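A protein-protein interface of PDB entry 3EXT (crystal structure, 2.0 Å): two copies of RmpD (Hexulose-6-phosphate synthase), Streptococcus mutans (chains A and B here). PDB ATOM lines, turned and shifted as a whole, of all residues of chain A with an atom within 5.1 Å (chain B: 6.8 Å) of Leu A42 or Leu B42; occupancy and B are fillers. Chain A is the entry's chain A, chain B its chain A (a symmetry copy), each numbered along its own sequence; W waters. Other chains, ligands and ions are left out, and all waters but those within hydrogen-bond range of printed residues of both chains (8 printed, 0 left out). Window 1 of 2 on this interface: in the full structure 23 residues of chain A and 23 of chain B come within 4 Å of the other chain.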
ATOM      1  N   THR A  38     -27.765 -35.504   3.072  1.00  0.00           N
ATOM      2  CA  THR A  38     -27.373 -34.359   2.212  1.00  0.00           C
ATOM      3  C   THR A  38     -28.028 -33.067   2.698  1.00  0.00           C
ATOM      4  O   THR A  38     -27.426 -31.964   2.639  1.00  0.00           O
ATOM      5  CB  THR A  38     -27.855 -34.566   0.748  1.00  0.00           C
ATOM      6  OG1 THR A  38     -27.635 -35.909   0.349  1.00  0.00           O
ATOM      7  CG2 THR A  38     -27.138 -33.609  -0.324  1.00  0.00           C
ATOM      8  N   VAL A  39     -29.300 -33.180   3.119  1.00  0.00           N
ATOM      9  CA  VAL A  39     -30.022 -31.991   3.640  1.00  0.00           C
ATOM     10  C   VAL A  39     -29.258 -31.359   4.810  1.00  0.00           C
ATOM     11  O   VAL A  39     -29.093 -30.117   4.876  1.00  0.00           O
ATOM     12  CB  VAL A  39     -31.459 -32.359   4.103  1.00  0.00           C
ATOM     13  CG1 VAL A  39     -32.116 -31.201   4.787  1.00  0.00           C
ATOM     14  CG2 VAL A  39     -32.276 -32.739   2.894  1.00  0.00           C
ATOM     15  N   CYS A  40     -28.754 -32.214   5.702  1.00  0.00           N
ATOM     16  CA  CYS A  40     -28.027 -31.763   6.883  1.00  0.00           C
ATOM     17  C   CYS A  40     -26.635 -31.173   6.487  1.00  0.00           C
ATOM     18  O   CYS A  40     -26.316 -30.094   6.877  1.00  0.00           O
ATOM     19  CB  CYS A  40     -27.903 -32.918   7.923  1.00  0.00           C
ATOM     20  SG  CYS A  40     -27.411 -32.231   9.524  1.00  0.00           S
ATOM     21  N   LEU A  41     -25.850 -31.881   5.684  1.00  0.00           N
ATOM     22  CA  LEU A  41     -24.529 -31.373   5.187  1.00  0.00           C
ATOM     23  C   LEU A  41     -24.586 -30.012   4.459  1.00  0.00           C
ATOM     24  O   LEU A  41     -23.759 -29.135   4.687  1.00  0.00           O
ATOM     25  CB  LEU A  41     -23.899 -32.447   4.279  1.00  0.00           C
ATOM     26  CG  LEU A  41     -23.493 -33.789   4.934  1.00  0.00           C
ATOM     27  CD1 LEU A  41     -22.935 -34.786   3.916  1.00  0.00           C
ATOM     28  CD2 LEU A  41     -22.390 -33.527   6.019  1.00  0.00           C
ATOM     29  N   LEU A  42     -25.614 -29.812   3.638  1.00  0.00           N
ATOM     30  CA  LEU A  42     -25.811 -28.513   2.946  1.00  0.00           C
ATOM     31  C   LEU A  42     -26.114 -27.386   3.939  1.00  0.00           C
ATOM     32  O   LEU A  42     -25.847 -26.203   3.676  1.00  0.00           O
ATOM     33  CB  LEU A  42     -26.917 -28.627   1.868  1.00  0.00           C
ATOM     34  CG  LEU A  42     -26.554 -29.498   0.661  1.00  0.00           C
ATOM     35  CD1 LEU A  42     -27.790 -29.840  -0.210  1.00  0.00           C
ATOM     36  CD2 LEU A  42     -25.332 -28.866  -0.197  1.00  0.00           C
ATOM     37  N   GLN A  43     -26.705 -27.754   5.068  1.00  0.00           N
ATOM     38  CA  GLN A  43     -26.986 -26.807   6.124  1.00  0.00           C
ATOM     39  C   GLN A  43     -25.792 -26.496   7.011  1.00  0.00           C
ATOM     40  O   GLN A  43     -25.586 -25.349   7.405  1.00  0.00           O
ATOM     41  CB  GLN A  43     -28.139 -27.307   7.031  1.00  0.00           C
ATOM     42  CG  GLN A  43     -29.551 -26.998   6.506  1.00  0.00           C
ATOM     43  CD  GLN A  43     -29.869 -25.502   6.377  1.00  0.00           C
ATOM     44  OE1 GLN A  43     -29.470 -24.845   5.416  1.00  0.00           O
ATOM     45  NE2 GLN A  43     -30.654 -24.982   7.303  1.00  0.00           N
ATOM     46  N   VAL A  44     -25.060 -27.541   7.413  1.00  0.00           N
ATOM     47  CA  VAL A  44     -24.088 -27.391   8.517  1.00  0.00           C
ATOM     48  C   VAL A  44     -22.656 -27.646   8.093  1.00  0.00           C
ATOM     49  O   VAL A  44     -21.740 -27.299   8.836  1.00  0.00           O
ATOM     50  CB  VAL A  44     -24.452 -28.313   9.772  1.00  0.00           C
ATOM     51  CG1 VAL A  44     -25.960 -28.243  10.094  1.00  0.00           C
ATOM     52  CG2 VAL A  44     -24.124 -29.688   9.549  1.00  0.00           C
ATOM     53  N   GLY A  45     -22.461 -28.252   6.912  1.00  0.00           N
ATOM     54  CA  GLY A  45     -21.079 -28.513   6.456  1.00  0.00           C
ATOM     55  C   GLY A  45     -20.484 -29.785   7.031  1.00  0.00           C
ATOM     56  O   GLY A  45     -21.159 -30.518   7.761  1.00  0.00           O
ATOM     57  N   SER A  46     -19.215 -30.067   6.702  1.00  0.00           N
ATOM     58  CA  SER A  46     -18.629 -31.373   6.994  1.00  0.00           C
ATOM     59  C   SER A  46     -18.138 -31.496   8.438  1.00  0.00           C
ATOM     60  O   SER A  46     -17.708 -32.596   8.814  1.00  0.00           O
ATOM     61  CB  SER A  46     -17.476 -31.678   5.980  1.00  0.00           C
ATOM     62  OG  SER A  46     -16.488 -30.656   6.100  1.00  0.00           O
ATOM     63  N   THR A  65     -23.124 -36.832   0.278  1.00  0.00           N
ATOM     64  CA  THR A  65     -22.935 -35.539  -0.423  1.00  0.00           C
ATOM     65  C   THR A  65     -23.601 -35.535  -1.800  1.00  0.00           C
ATOM     66  O   THR A  65     -23.773 -34.452  -2.416  1.00  0.00           O
ATOM     67  CB  THR A  65     -21.422 -35.283  -0.677  1.00  0.00           C
ATOM     68  OG1 THR A  65     -20.886 -36.406  -1.385  1.00  0.00           O
ATOM     69  CG2 THR A  65     -20.650 -35.082   0.685  1.00  0.00           C
ATOM     70  N   VAL A  74     -14.272 -33.268  -3.064  1.00  0.00           N
ATOM     71  CA  VAL A  74     -15.368 -33.509  -2.094  1.00  0.00           C
ATOM     72  C   VAL A  74     -15.087 -34.739  -1.234  1.00  0.00           C
ATOM     73  O   VAL A  74     -15.358 -34.766   0.006  1.00  0.00           O
ATOM     74  CB  VAL A  74     -16.774 -33.586  -2.794  1.00  0.00           C
ATOM     75  CG1 VAL A  74     -17.863 -33.882  -1.761  1.00  0.00           C
ATOM     76  CG2 VAL A  74     -17.104 -32.243  -3.522  1.00  0.00           C
ATOM     77  N   GLY B  37     -20.593 -22.274  -4.434  1.00  0.00           N
ATOM     78  CA  GLY B  37     -20.489 -23.500  -5.203  1.00  0.00           C
ATOM     79  C   GLY B  37     -20.701 -24.718  -4.289  1.00  0.00           C
ATOM     80  O   GLY B  37     -20.594 -24.594  -3.051  1.00  0.00           O
ATOM     81  N   THR B  38     -21.057 -25.861  -4.879  1.00  0.00           N
ATOM     82  CA  THR B  38     -21.474 -27.049  -4.093  1.00  0.00           C
ATOM     83  C   THR B  38     -20.342 -27.521  -3.182  1.00  0.00           C
ATOM     84  O   THR B  38     -20.573 -27.986  -2.036  1.00  0.00           O
ATOM     85  CB  THR B  38     -21.810 -28.247  -5.024  1.00  0.00           C
ATOM     86  OG1 THR B  38     -22.550 -27.798  -6.147  1.00  0.00           O
ATOM     87  CG2 THR B  38     -22.652 -29.418  -4.316  1.00  0.00           C
ATOM     88  N   VAL B  39     -19.107 -27.472  -3.712  1.00  0.00           N
ATOM     89  CA  VAL B  39     -17.931 -27.880  -2.902  1.00  0.00           C
ATOM     90  C   VAL B  39     -17.852 -27.064  -1.605  1.00  0.00           C
ATOM     91  O   VAL B  39     -17.620 -27.622  -0.506  1.00  0.00           O
ATOM     92  CB  VAL B  39     -16.608 -27.708  -3.699  1.00  0.00           C
ATOM     93  CG1 VAL B  39     -15.418 -27.950  -2.823  1.00  0.00           C
ATOM     94  CG2 VAL B  39     -16.591 -28.703  -4.831  1.00  0.00           C
ATOM     95  N   CYS B  40     -18.094 -25.758  -1.727  1.00  0.00           N
ATOM     96  CA  CYS B  40     -18.029 -24.848  -0.590  1.00  0.00           C
ATOM     97  C   CYS B  40     -19.222 -25.095   0.389  1.00  0.00           C
ATOM     98  O   CYS B  40     -19.012 -25.265   1.549  1.00  0.00           O
ATOM     99  CB  CYS B  40     -17.963 -23.368  -1.076  1.00  0.00           C
ATOM    100  SG  CYS B  40     -17.440 -22.310   0.296  1.00  0.00           S
ATOM    101  N   LEU B  41     -20.451 -25.152  -0.109  1.00  0.00           N
ATOM    102  CA  LEU B  41     -21.654 -25.456   0.733  1.00  0.00           C
ATOM    103  C   LEU B  41     -21.574 -26.776   1.531  1.00  0.00           C
ATOM    104  O   LEU B  41     -21.921 -26.830   2.707  1.00  0.00           O
ATOM    105  CB  LEU B  41     -22.902 -25.446  -0.170  1.00  0.00           C
ATOM    106  CG  LEU B  41     -23.306 -24.099  -0.817  1.00  0.00           C
ATOM    107  CD1 LEU B  41     -24.524 -24.237  -1.733  1.00  0.00           C
ATOM    108  CD2 LEU B  41     -23.654 -23.063   0.309  1.00  0.00           C
ATOM    109  N   LEU B  42     -21.038 -27.823   0.909  1.00  0.00           N
ATOM    110  CA  LEU B  42     -20.840 -29.120   1.605  1.00  0.00           C
ATOM    111  C   LEU B  42     -19.812 -29.002   2.734  1.00  0.00           C
ATOM    112  O   LEU B  42     -19.834 -29.764   3.713  1.00  0.00           O
ATOM    113  CB  LEU B  42     -20.445 -30.229   0.599  1.00  0.00           C
ATOM    114  CG  LEU B  42     -21.554 -30.639  -0.377  1.00  0.00           C
ATOM    115  CD1 LEU B  42     -21.016 -31.497  -1.551  1.00  0.00           C
ATOM    116  CD2 LEU B  42     -22.808 -31.328   0.386  1.00  0.00           C
ATOM    117  N   GLN B  43     -18.888 -28.062   2.579  1.00  0.00           N
ATOM    118  CA  GLN B  43     -17.898 -27.791   3.598  1.00  0.00           C
ATOM    119  C   GLN B  43     -18.402 -26.915   4.733  1.00  0.00           C
ATOM    120  O   GLN B  43     -18.076 -27.148   5.896  1.00  0.00           O
ATOM    121  CB  GLN B  43     -16.643 -27.114   2.992  1.00  0.00           C
ATOM    122  CG  GLN B  43     -15.617 -28.087   2.387  1.00  0.00           C
ATOM    123  CD  GLN B  43     -15.000 -29.069   3.392  1.00  0.00           C
ATOM    124  OE1 GLN B  43     -15.604 -30.078   3.752  1.00  0.00           O
ATOM    125  NE2 GLN B  43     -13.764 -28.815   3.785  1.00  0.00           N
ATOM    126  N   VAL B  44     -19.116 -25.839   4.384  1.00  0.00           N
ATOM    127  CA  VAL B  44     -19.375 -24.765   5.366  1.00  0.00           C
ATOM    128  C   VAL B  44     -20.847 -24.578   5.675  1.00  0.00           C
ATOM    129  O   VAL B  44     -21.175 -23.913   6.656  1.00  0.00           O
ATOM    130  CB  VAL B  44     -18.736 -23.369   4.919  1.00  0.00           C
ATOM    131  CG1 VAL B  44     -17.300 -23.561   4.389  1.00  0.00           C
ATOM    132  CG2 VAL B  44     -19.494 -22.732   3.885  1.00  0.00           C
ATOM    133  N   GLY B  45     -21.730 -25.153   4.844  1.00  0.00           N
ATOM    134  CA  GLY B  45     -23.175 -25.002   5.111  1.00  0.00           C
ATOM    135  C   GLY B  45     -23.756 -23.705   4.580  1.00  0.00           C
ATOM    136  O   GLY B  45     -23.048 -22.916   3.945  1.00  0.00           O
ATOM    137  N   SER B  46     -25.054 -23.472   4.825  1.00  0.00           N
ATOM    138  CA  SER B  46     -25.768 -22.386   4.158  1.00  0.00           C
ATOM    139  C   SER B  46     -25.539 -21.027   4.821  1.00  0.00           C
ATOM    140  O   SER B  46     -26.026 -20.025   4.277  1.00  0.00           O
ATOM    141  CB  SER B  46     -27.295 -22.723   4.077  1.00  0.00           C
ATOM    142  OG  SER B  46     -27.789 -22.896   5.404  1.00  0.00           O
ATOM    143  N   GLU B  47     -24.796 -20.929   5.942  1.00  0.00           N
ATOM    144  CA  GLU B  47     -24.572 -19.590   6.509  1.00  0.00           C
ATOM    145  C   GLU B  47     -23.796 -18.699   5.533  1.00  0.00           C
ATOM    146  O   GLU B  47     -23.956 -17.455   5.545  1.00  0.00           O
ATOM    147  CB  GLU B  47     -23.886 -19.609   7.870  1.00  0.00           C
ATOM    148  CG  GLU B  47     -24.133 -18.270   8.585  1.00  0.00           C
ATOM    149  CD  GLU B  47     -23.505 -18.183   9.964  1.00  0.00           C
ATOM    150  OE1 GLU B  47     -22.632 -19.019  10.313  1.00  0.00           O
ATOM    151  OE2 GLU B  47     -23.872 -17.232  10.698  1.00  0.00           O
ATOM    152  N   ASP B  64     -25.589 -23.209  -5.093  1.00  0.00           N
ATOM    153  CA  ASP B  64     -25.406 -24.362  -5.974  1.00  0.00           C
ATOM    154  C   ASP B  64     -25.432 -25.658  -5.162  1.00  0.00           C
ATOM    155  O   ASP B  64     -24.382 -26.257  -4.879  1.00  0.00           O
ATOM    156  CB  ASP B  64     -24.068 -24.183  -6.735  1.00  0.00           C
ATOM    157  CG  ASP B  64     -23.801 -25.262  -7.740  1.00  0.00           C
ATOM    158  OD1 ASP B  64     -24.685 -26.085  -8.062  1.00  0.00           O
ATOM    159  OD2 ASP B  64     -22.627 -25.337  -8.194  1.00  0.00           O
ATOM    160  N   THR B  65     -26.627 -26.129  -4.807  1.00  0.00           N
ATOM    161  CA  THR B  65     -26.759 -27.325  -3.938  1.00  0.00           C
ATOM    162  C   THR B  65     -26.842 -28.615  -4.754  1.00  0.00           C
ATOM    163  O   THR B  65     -26.688 -29.730  -4.191  1.00  0.00           O
ATOM    164  CB  THR B  65     -28.079 -27.249  -3.119  1.00  0.00           C
ATOM    165  OG1 THR B  65     -29.169 -27.077  -4.032  1.00  0.00           O
ATOM    166  CG2 THR B  65     -28.036 -26.049  -2.095  1.00  0.00           C
ATOM    167  N   LYS B  66     -27.077 -28.488  -6.068  1.00  0.00           N
ATOM    168  CA  LYS B  66     -27.334 -29.653  -6.951  1.00  0.00           C
ATOM    169  C   LYS B  66     -28.333 -30.589  -6.279  1.00  0.00           C
ATOM    170  O   LYS B  66     -28.106 -31.784  -6.198  1.00  0.00           O
ATOM    171  CB  LYS B  66     -26.049 -30.412  -7.274  1.00  0.00           C
ATOM    172  CG  LYS B  66     -25.199 -29.663  -8.329  1.00  0.00           C
ATOM    173  CD  LYS B  66     -23.802 -30.226  -8.448  1.00  0.00           C
ATOM    174  CE  LYS B  66     -22.957 -29.454  -9.509  1.00  0.00           C
ATOM    175  NZ  LYS B  66     -22.577 -28.070  -9.049  1.00  0.00           N
ATOM    176  N   CYS B  67     -29.450 -30.030  -5.840  1.00  0.00           N
ATOM    177  CA  CYS B  67     -30.459 -30.796  -5.093  1.00  0.00           C
ATOM    178  C   CYS B  67     -30.981 -31.991  -5.927  1.00  0.00           C
ATOM    179  O   CYS B  67     -31.388 -31.801  -7.061  1.00  0.00           O
ATOM    180  CB  CYS B  67     -31.580 -29.833  -4.793  1.00  0.00           C
ATOM    181  SG  CYS B  67     -32.946 -30.510  -3.897  1.00  0.00           S
ATOM    182  N   VAL B  74     -34.650 -28.270   0.962  1.00  0.00           N
ATOM    183  CA  VAL B  74     -33.342 -27.664   0.613  1.00  0.00           C
ATOM    184  C   VAL B  74     -33.514 -26.246   0.074  1.00  0.00           C
ATOM    185  O   VAL B  74     -32.714 -25.310   0.383  1.00  0.00           O
ATOM    186  CB  VAL B  74     -32.509 -28.571  -0.364  1.00  0.00           C
ATOM    187  CG1 VAL B  74     -31.192 -27.884  -0.729  1.00  0.00           C
ATOM    188  CG2 VAL B  74     -32.204 -29.956   0.292  1.00  0.00           C
ATOM    189  N   ASN B  77     -34.362 -23.940   2.954  1.00  0.00           N
ATOM    190  CA  ASN B  77     -33.174 -23.736   3.756  1.00  0.00           C
ATOM    191  C   ASN B  77     -32.268 -22.659   3.135  1.00  0.00           C
ATOM    192  O   ASN B  77     -31.665 -21.846   3.859  1.00  0.00           O
ATOM    193  CB  ASN B  77     -32.385 -25.067   3.999  1.00  0.00           C
ATOM    194  CG  ASN B  77     -33.101 -25.996   4.990  1.00  0.00           C
ATOM    195  OD1 ASN B  77     -34.064 -25.564   5.618  1.00  0.00           O
ATOM    196  ND2 ASN B  77     -32.674 -27.288   5.094  1.00  0.00           N
ATOM    197  N   ASN B  78     -32.167 -22.655   1.821  1.00  0.00           N
ATOM    198  CA  ASN B  78     -31.284 -21.670   1.144  1.00  0.00           C
ATOM    199  C   ASN B  78     -31.956 -20.338   0.837  1.00  0.00           C
ATOM    200  O   ASN B  78     -31.318 -19.290   0.904  1.00  0.00           O
ATOM    201  CB  ASN B  78     -30.660 -22.290  -0.111  1.00  0.00           C
ATOM    202  CG  ASN B  78     -29.630 -23.331   0.253  1.00  0.00           C
ATOM    203  OD1 ASN B  78     -28.492 -22.980   0.544  1.00  0.00           O
ATOM    204  ND2 ASN B  78     -30.062 -24.596   0.383  1.00  0.00           N
HETATM  205  O   HOH W   1     -26.834 -25.215   1.218  1.00  0.00           O
HETATM  206  O   HOH W   2     -27.315 -23.632   8.731  1.00  0.00           O
HETATM  207  O   HOH W   3     -23.476 -22.990   7.781  1.00  0.00           O
HETATM  208  O   HOH W   4     -30.618 -28.311   3.257  1.00  0.00           O
HETATM  209  O   HOH W   5     -15.532 -27.465   6.956  1.00  0.00           O
HETATM  210  O   HOH W   6     -31.480 -22.158   6.793  1.00  0.00           O
HETATM  211  O   HOH W   7     -29.191 -26.119   2.833  1.00  0.00           O
HETATM  212  O   HOH W   8     -19.027 -27.514   8.917  1.00  0.00           O
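The backbone carbonyl oxygen (O) of Leu A42 is in hydrogen-bond range of the backbone NH (N) of Ser B46, 3.1 Å away. The side-chain amide oxygen of Gln A43 lies within hydrogen-bond range of the side-chain hydroxyl of Ser B46 (2.6 Å). N of Ser A46 sits at hydrogen-bond distance from O of Leu B42 (3.1 Å). The side-chain hydroxyl (OG) of Ser A46 lies within hydrogen-bond range of the side-chain amide oxygen (OE1) of Gln B43.
The backbone NH (N) of Cys B67 sits close to the side-chain hydroxyl (OG1) of Thr B65 (3.5 Å). ND2 of Asn B78 lies within hydrogen-bond range of O of Val B74 (2.7 Å).
Leu A41 touches Leu B41 (O to O, 3.6 Å). Leu A42 touches Leu B42. Thr B65 touches Leu A42. Val B74 touches Leu A42 (CG1 to CD1, 3.96 Å). Gly B45 touches Gln A43. Gln A43 touches Asn B77 (OE1 to CB, 3.2 Å). Gly A45 touches Leu B42. Gly A45 touches Gln B43. Leu B42 touches Thr A65 (CD1 to CB, 3.9 Å). CG1 of Val A74 touches CD1 of Leu B42 (3.96 Å).
Leu B42 touches just these residues of chain A: Leu A42 (3.6 Å), Gly A45 (3.3 Å), Ser A46 (3.1 Å), Thr A65 (3.9 Å) and Val A74 (3.96 Å). Of the printed residues of chain B, Thr A65 touches Leu B42 (3.9 Å). Of the printed residues of chain A, Val B74 touches Val A39 (3.8 Å) and Leu A42 (3.96 Å). Cys B40 touches none of the printed residues of chain A. Glu B47 touches none of the printed residues of chain A. The nearest residue of chain A that does not touch Leu B42 is Leu A41 (4.1 Å). The nearest printed residue of chain A that does not touch Val B44 is Val A44 (4.1 Å).
Of the 18 printed residues of chain B, 10 touch a printed residue of chain A. Hydrophobic or aromatic side chains of chain B within 4 Å of the printed part of chain A: Val B39, Leu B42 and Val B74. Along chain B the printed residues that touch a printed residue of chain A span positions 39 to 77. Of the 11 printed residues of chain A, 9 touch a printed residue of chain B. Hydrophobic or aromatic side chains of chain A within 4 Å of the printed part of chain B: Val A39, Leu A42 and Val A74. Among the printed residues, 21 pairs touch across the chains. Among the printed residues, no Asp or Glu carboxylate lies within 4 Å of a Lys or Arg side-chain nitrogen of the other chain.
Val A39 touches Val B74, and with the chains exchanged Val A74 touches Val B39. Leu A42 touches Ser B46, and with the chains exchanged Ser A46 touches Leu B42. Leu A42 touches Thr B65, and with the chains exchanged Thr A65 touches Leu B42. Gln A43 touches Ser B46, and with the chains exchanged Ser A46 touches Gln B43. Positions printed for both chains: 38, 39, 40, 41, 42, 43, 44, 45, 46, 65 and 74. Of the 21 pairs that touch across the chains among the printed residues, 19 have their exchanged pair printed and touching as well.
Water W8 lies within hydrogen-bond range of O of Val A44, O of Gln B43 and N of Ser A46. Water W3 lies within hydrogen-bond range of the backbone carbonyl oxygen of Val B44 (2.7 Å), the backbone NH of Glu B47 (3.1 Å), the backbone carbonyl oxygen of Gln A43 (3.2 Å) and the backbone NH of Ser B46 (3.4 Å). Water W2 bridges O of Gln A43 (2.8 Å) and OG of Ser B46 (3.4 Å). Water W1 bridges O of Leu A42 (2.8 Å) and OD1 of Asn B78 (2.9 Å). Water W4 lies within hydrogen-bond range of the backbone carbonyl oxygen of Val A39 (2.9 Å) and the side-chain amide nitrogen of Asn B77 (2.9 Å). Water W6 lies within hydrogen-bond range of O of Asn B77 (3.0 Å) and NE2 of Gln A43 (3.0 Å).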
